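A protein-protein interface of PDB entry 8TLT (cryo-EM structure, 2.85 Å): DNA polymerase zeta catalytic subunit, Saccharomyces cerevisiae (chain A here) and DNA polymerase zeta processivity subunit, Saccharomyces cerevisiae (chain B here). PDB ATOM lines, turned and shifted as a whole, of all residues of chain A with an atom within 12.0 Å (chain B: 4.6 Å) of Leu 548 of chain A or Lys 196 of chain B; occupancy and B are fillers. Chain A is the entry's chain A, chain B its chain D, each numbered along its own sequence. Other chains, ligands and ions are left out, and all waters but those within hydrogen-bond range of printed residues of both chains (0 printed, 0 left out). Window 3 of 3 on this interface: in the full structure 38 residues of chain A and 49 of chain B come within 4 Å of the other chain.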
ATOM      1  N   GLY A 547       7.523 -11.570 -28.066  1.00  0.00           N
ATOM      2  CA  GLY A 547       6.717 -12.390 -27.181  1.00  0.00           C
ATOM      3  C   GLY A 547       5.572 -11.634 -26.540  1.00  0.00           C
ATOM      4  O   GLY A 547       5.756 -10.529 -26.030  1.00  0.00           O
ATOM      5  N   LEU A 548       4.384 -12.231 -26.569  1.00  0.00           N
ATOM      6  CA  LEU A 548       3.211 -11.589 -25.993  1.00  0.00           C
ATOM      7  C   LEU A 548       3.328 -11.520 -24.476  1.00  0.00           C
ATOM      8  O   LEU A 548       3.736 -12.484 -23.822  1.00  0.00           O
ATOM      9  CB  LEU A 548       1.945 -12.347 -26.390  1.00  0.00           C
ATOM     10  CG  LEU A 548       1.936 -12.945 -27.799  1.00  0.00           C
ATOM     11  CD1 LEU A 548       0.842 -13.987 -27.934  1.00  0.00           C
ATOM     12  CD2 LEU A 548       1.769 -11.854 -28.840  1.00  0.00           C
ATOM     13  N   ARG A 549       2.965 -10.369 -23.916  1.00  0.00           N
ATOM     14  CA  ARG A 549       3.034 -10.184 -22.474  1.00  0.00           C
ATOM     15  C   ARG A 549       1.932 -10.976 -21.781  1.00  0.00           C
ATOM     16  O   ARG A 549       0.802 -11.058 -22.268  1.00  0.00           O
ATOM     17  CB  ARG A 549       2.920  -8.702 -22.121  1.00  0.00           C
ATOM     18  CG  ARG A 549       2.599  -7.803 -23.302  1.00  0.00           C
ATOM     19  N   TYR A 550       2.272 -11.566 -20.634  1.00  0.00           N
ATOM     20  CA  TYR A 550       1.305 -12.387 -19.913  1.00  0.00           C
ATOM     21  C   TYR A 550       0.184 -11.541 -19.319  1.00  0.00           C
ATOM     22  O   TYR A 550      -0.983 -11.947 -19.342  1.00  0.00           O
ATOM     23  CB  TYR A 550       2.012 -13.193 -18.825  1.00  0.00           C
ATOM     24  CG  TYR A 550       2.837 -14.339 -19.363  1.00  0.00           C
ATOM     25  CD1 TYR A 550       2.395 -15.087 -20.445  1.00  0.00           C
ATOM     26  CD2 TYR A 550       4.055 -14.675 -18.788  1.00  0.00           C
ATOM     27  CE1 TYR A 550       3.143 -16.135 -20.944  1.00  0.00           C
ATOM     28  CE2 TYR A 550       4.809 -15.724 -19.279  1.00  0.00           C
ATOM     29  CZ  TYR A 550       4.348 -16.449 -20.356  1.00  0.00           C
ATOM     30  N   GLY A 551       0.513 -10.380 -18.783  1.00  0.00           N
ATOM     31  CA  GLY A 551      -0.496  -9.494 -18.238  1.00  0.00           C
ATOM     32  C   GLY A 551       0.061  -8.691 -17.080  1.00  0.00           C
ATOM     33  O   GLY A 551       1.206  -8.854 -16.669  1.00  0.00           O
ATOM     34  N   LYS A 552      -0.792  -7.803 -16.562  1.00  0.00           N
ATOM     35  CA  LYS A 552      -0.399  -6.971 -15.430  1.00  0.00           C
ATOM     36  C   LYS A 552      -0.164  -7.809 -14.179  1.00  0.00           C
ATOM     37  O   LYS A 552       0.792  -7.567 -13.433  1.00  0.00           O
ATOM     38  CB  LYS A 552      -1.461  -5.903 -15.170  1.00  0.00           C
ATOM     39  N   ARG A 553      -1.024  -8.798 -13.932  1.00  0.00           N
ATOM     40  CA  ARG A 553      -0.903  -9.682 -12.768  1.00  0.00           C
ATOM     41  C   ARG A 553      -1.223 -11.096 -13.250  1.00  0.00           C
ATOM     42  O   ARG A 553      -2.385 -11.506 -13.280  1.00  0.00           O
ATOM     43  CB  ARG A 553      -1.825  -9.241 -11.640  1.00  0.00           C
ATOM     44  CG  ARG A 553      -1.829 -10.167 -10.436  1.00  0.00           C
ATOM     45  N   ALA A 554      -0.183 -11.838 -13.623  1.00  0.00           N
ATOM     46  CA  ALA A 554      -0.332 -13.151 -14.228  1.00  0.00           C
ATOM     47  C   ALA A 554       0.368 -14.206 -13.385  1.00  0.00           C
ATOM     48  O   ALA A 554       1.491 -13.997 -12.917  1.00  0.00           O
ATOM     49  CB  ALA A 554       0.229 -13.169 -15.651  1.00  0.00           C
ATOM     50  N   PHE A 555      -0.302 -15.339 -13.201  1.00  0.00           N
ATOM     51  CA  PHE A 555       0.238 -16.481 -12.482  1.00  0.00           C
ATOM     52  C   PHE A 555       0.537 -17.605 -13.464  1.00  0.00           C
ATOM     53  O   PHE A 555      -0.148 -17.764 -14.478  1.00  0.00           O
ATOM     54  CB  PHE A 555      -0.736 -16.971 -11.405  1.00  0.00           C
ATOM     55  CG  PHE A 555      -0.820 -16.072 -10.201  1.00  0.00           C
ATOM     56  CD1 PHE A 555      -0.162 -14.854 -10.173  1.00  0.00           C
ATOM     57  CD2 PHE A 555      -1.564 -16.448  -9.095  1.00  0.00           C
ATOM     58  CE1 PHE A 555      -0.242 -14.031  -9.066  1.00  0.00           C
ATOM     59  CE2 PHE A 555      -1.648 -15.628  -7.985  1.00  0.00           C
ATOM     60  CZ  PHE A 555      -0.985 -14.418  -7.972  1.00  0.00           C
ATOM     61  N   VAL A 556       1.569 -18.385 -13.156  1.00  0.00           N
ATOM     62  CA  VAL A 556       2.054 -19.446 -14.030  1.00  0.00           C
ATOM     63  C   VAL A 556       1.849 -20.782 -13.334  1.00  0.00           C
ATOM     64  O   VAL A 556       2.220 -20.945 -12.165  1.00  0.00           O
ATOM     65  CB  VAL A 556       3.534 -19.237 -14.395  1.00  0.00           C
ATOM     66  CG1 VAL A 556       3.873 -19.980 -15.669  1.00  0.00           C
ATOM     67  CG2 VAL A 556       3.839 -17.755 -14.542  1.00  0.00           C
ATOM     68  N   CYS B  87       6.308 -16.250 -26.081  1.00  0.00           N
ATOM     69  CA  CYS B  87       4.925 -16.681 -26.267  1.00  0.00           C
ATOM     70  C   CYS B  87       4.524 -16.415 -27.712  1.00  0.00           C
ATOM     71  O   CYS B  87       4.171 -15.291 -28.076  1.00  0.00           O
ATOM     72  CB  CYS B  87       4.006 -15.959 -25.290  1.00  0.00           C
ATOM     73  SG  CYS B  87       2.346 -16.652 -25.174  1.00  0.00           S
ATOM     74  N   ILE B  88       4.587 -17.454 -28.546  1.00  0.00           N
ATOM     75  CA  ILE B  88       4.234 -17.301 -29.954  1.00  0.00           C
ATOM     76  C   ILE B  88       2.736 -17.072 -30.113  1.00  0.00           C
ATOM     77  O   ILE B  88       2.302 -16.172 -30.841  1.00  0.00           O
ATOM     78  CB  ILE B  88       4.705 -18.526 -30.758  1.00  0.00           C
ATOM     79  CG1 ILE B  88       6.180 -18.809 -30.477  1.00  0.00           C
ATOM     80  CG2 ILE B  88       4.481 -18.307 -32.242  1.00  0.00           C
ATOM     81  N   GLU B  89       1.923 -17.880 -29.434  1.00  0.00           N
ATOM     82  CA  GLU B  89       0.475 -17.811 -29.544  1.00  0.00           C
ATOM     83  C   GLU B  89      -0.148 -17.809 -28.156  1.00  0.00           C
ATOM     84  O   GLU B  89       0.455 -18.260 -27.181  1.00  0.00           O
ATOM     85  CB  GLU B  89      -0.097 -18.981 -30.357  1.00  0.00           C
ATOM     86  CG  GLU B  89       0.689 -19.336 -31.602  1.00  0.00           C
ATOM     87  CD  GLU B  89       0.216 -20.629 -32.235  1.00  0.00           C
ATOM     88  N   LYS B  90      -1.372 -17.294 -28.084  1.00  0.00           N
ATOM     89  CA  LYS B  90      -2.122 -17.259 -26.838  1.00  0.00           C
ATOM     90  C   LYS B  90      -3.598 -17.442 -27.154  1.00  0.00           C
ATOM     91  O   LYS B  90      -4.081 -16.960 -28.181  1.00  0.00           O
ATOM     92  CB  LYS B  90      -1.892 -15.945 -26.086  1.00  0.00           C
ATOM     93  CG  LYS B  90      -2.143 -16.030 -24.594  1.00  0.00           C
ATOM     94  CD  LYS B  90      -1.358 -14.967 -23.845  1.00  0.00           C
ATOM     95  CE  LYS B  90      -1.974 -13.592 -24.026  1.00  0.00           C
ATOM     96  NZ  LYS B  90      -2.336 -12.974 -22.720  1.00  0.00           N
ATOM     97  N   LYS B 196       4.074  -6.713 -31.766  1.00  0.00           N
ATOM     98  CA  LYS B 196       3.108  -7.103 -32.786  1.00  0.00           C
ATOM     99  C   LYS B 196       2.103  -8.107 -32.231  1.00  0.00           C
ATOM    100  O   LYS B 196       2.433  -8.913 -31.362  1.00  0.00           O
ATOM    101  CB  LYS B 196       3.821  -7.690 -34.004  1.00  0.00           C
ATOM    102  N   ILE B 197       0.872  -8.054 -32.740  1.00  0.00           N
ATOM    103  CA  ILE B 197      -0.191  -8.943 -32.285  1.00  0.00           C
ATOM    104  C   ILE B 197      -1.207  -9.070 -33.408  1.00  0.00           C
ATOM    105  O   ILE B 197      -1.338  -8.179 -34.250  1.00  0.00           O
ATOM    106  CB  ILE B 197      -0.832  -8.421 -30.972  1.00  0.00           C
ATOM    107  CG1 ILE B 197      -0.944  -9.549 -29.946  1.00  0.00           C
ATOM    108  CG2 ILE B 197      -2.191  -7.785 -31.235  1.00  0.00           C
ATOM    109  N   GLU B 217      -4.456 -14.610 -29.933  1.00  0.00           N
ATOM    110  CA  GLU B 217      -3.452 -13.685 -30.435  1.00  0.00           C
ATOM    111  C   GLU B 217      -2.304 -14.472 -31.050  1.00  0.00           C
ATOM    112  O   GLU B 217      -2.107 -15.654 -30.760  1.00  0.00           O
ATOM    113  CB  GLU B 217      -2.926 -12.761 -29.328  1.00  0.00           C
ATOM    114  CG  GLU B 217      -3.538 -13.012 -27.962  1.00  0.00           C
ATOM    115  N   LYS B 218      -1.544 -13.800 -31.911  1.00  0.00           N
ATOM    116  CA  LYS B 218      -0.454 -14.438 -32.634  1.00  0.00           C
ATOM    117  C   LYS B 218       0.743 -13.499 -32.684  1.00  0.00           C
ATOM    118  O   LYS B 218       0.617 -12.286 -32.502  1.00  0.00           O
ATOM    119  CB  LYS B 218      -0.882 -14.835 -34.053  1.00  0.00           C
ATOM    120  CG  LYS B 218      -0.059 -15.952 -34.671  1.00  0.00           C
ATOM    121  CD  LYS B 218      -0.956 -17.012 -35.282  1.00  0.00           C
ATOM    122  CE  LYS B 218      -1.660 -16.484 -36.521  1.00  0.00           C
ATOM    123  NZ  LYS B 218      -2.827 -17.327 -36.903  1.00  0.00           N
ATOM    124  N   LEU B 219       1.915 -14.087 -32.922  1.00  0.00           N
ATOM    125  CA  LEU B 219       3.173 -13.354 -33.065  1.00  0.00           C
ATOM    126  C   LEU B 219       3.486 -12.506 -31.837  1.00  0.00           C
ATOM    127  O   LEU B 219       4.646 -12.374 -31.443  1.00  0.00           O
ATOM    128  CB  LEU B 219       3.141 -12.473 -34.316  1.00  0.00           C
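Hydrophobic or aromatic side chains of chain B within 4 Å of the printed part of chain A: Ile 197.
Of the 10 printed residues of chain A, 4 touch a printed residue of chain B.
Printed residues of chain A that touch a printed residue of chain B: Gly 547, Leu 548, Arg 549 and Tyr 550.
Hydrophobic or aromatic side chains of chain A within 4 Å of the printed part of chain B: Leu 548.
Among the printed residues, 11 pairs touch across the chains.
Among the printed residues, no Asp or Glu carboxylate lies within 4 Å of a Lys or Arg side-chain nitrogen of the other chain.
Of the printed residues of chain B, Gly 547 of chain A touches Cys 87 (3.96 Å).
Of chain B, only Cys 87 (3.3 Å), Ile 88 (3.9 Å), Glu 89 (3.95 Å), Lys 90 (3.8 Å), Lys 196 (3.9 Å), Ile 197 (3.7 Å), Lys 218 (3.9 Å) and Leu 219 (3.5 Å) come within 4 Å of Leu 548 of chain A.
Of the printed residues of chain B, Arg 549 of chain A touches Lys 90 (3.7 Å).
Of the printed residues of chain B, Tyr 550 of chain A touches Lys 90.
Gly 551 of chain A touches none of the printed residues of chain B.
Ile 88 of chain B touches just one residue of chain A: Leu 548 (3.9 Å).
Glu 89 of chain B touches just one residue of chain A: Leu 548 (3.95 Å).
Of chain A, only Leu 548 comes within 4 Å of Ile 197 of chain B.
Of the printed residues of chain A, Lys 218 of chain B touches Leu 548.
Leu 219 of chain B touches just one residue of chain A: Leu 548 (3.5 Å).
The nearest residue of chain A that does not touch Lys 196 of chain B is Gly 547 of chain A (6.4 Å).
O of Glu 89 of chain B is in hydrogen-bond range of SG of Cys 87 of chain B, 3.2 Å away.
The backbone NH (N) of Glu 217 of chain B lies within hydrogen-bond range of the backbone carbonyl oxygen (O) of Lys 90 of chain B, at 3.0 Å.
The backbone NH (N) of Leu 219 of chain B is in hydrogen-bond range of the backbone carbonyl oxygen (O) of Ile 88 of chain B (3.0 Å).
Among the printed residues, pairs that only touch across the chains: Leu 548 of chain A with Leu 219 of chain B (3.5 Å), Arg 549 of chain A with Lys 90 of chain B (3.7 Å), Leu 548 of chain A with Ile 197 of chain B (3.7 Å), Tyr 550 of chain A with Lys 90 of chain B (3.8 Å), Leu 548 of chain A with Lys 90 of chain B (3.8 Å), Leu 548 of chain A with Lys 218 of chain B (3.9 Å), Leu 548 of chain A with Ile 88 of chain B (3.9 Å), Leu 548 of chain A with Lys 196 of chain B (3.9 Å), Leu 548 of chain A with Glu 89 of chain B (3.95 Å) and Gly 547 of chain A with Cys 87 of chain B (3.96 Å).
O of Cys 87 of chain B sits close to N of Leu 548 of chain A, 3.4 Å away.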
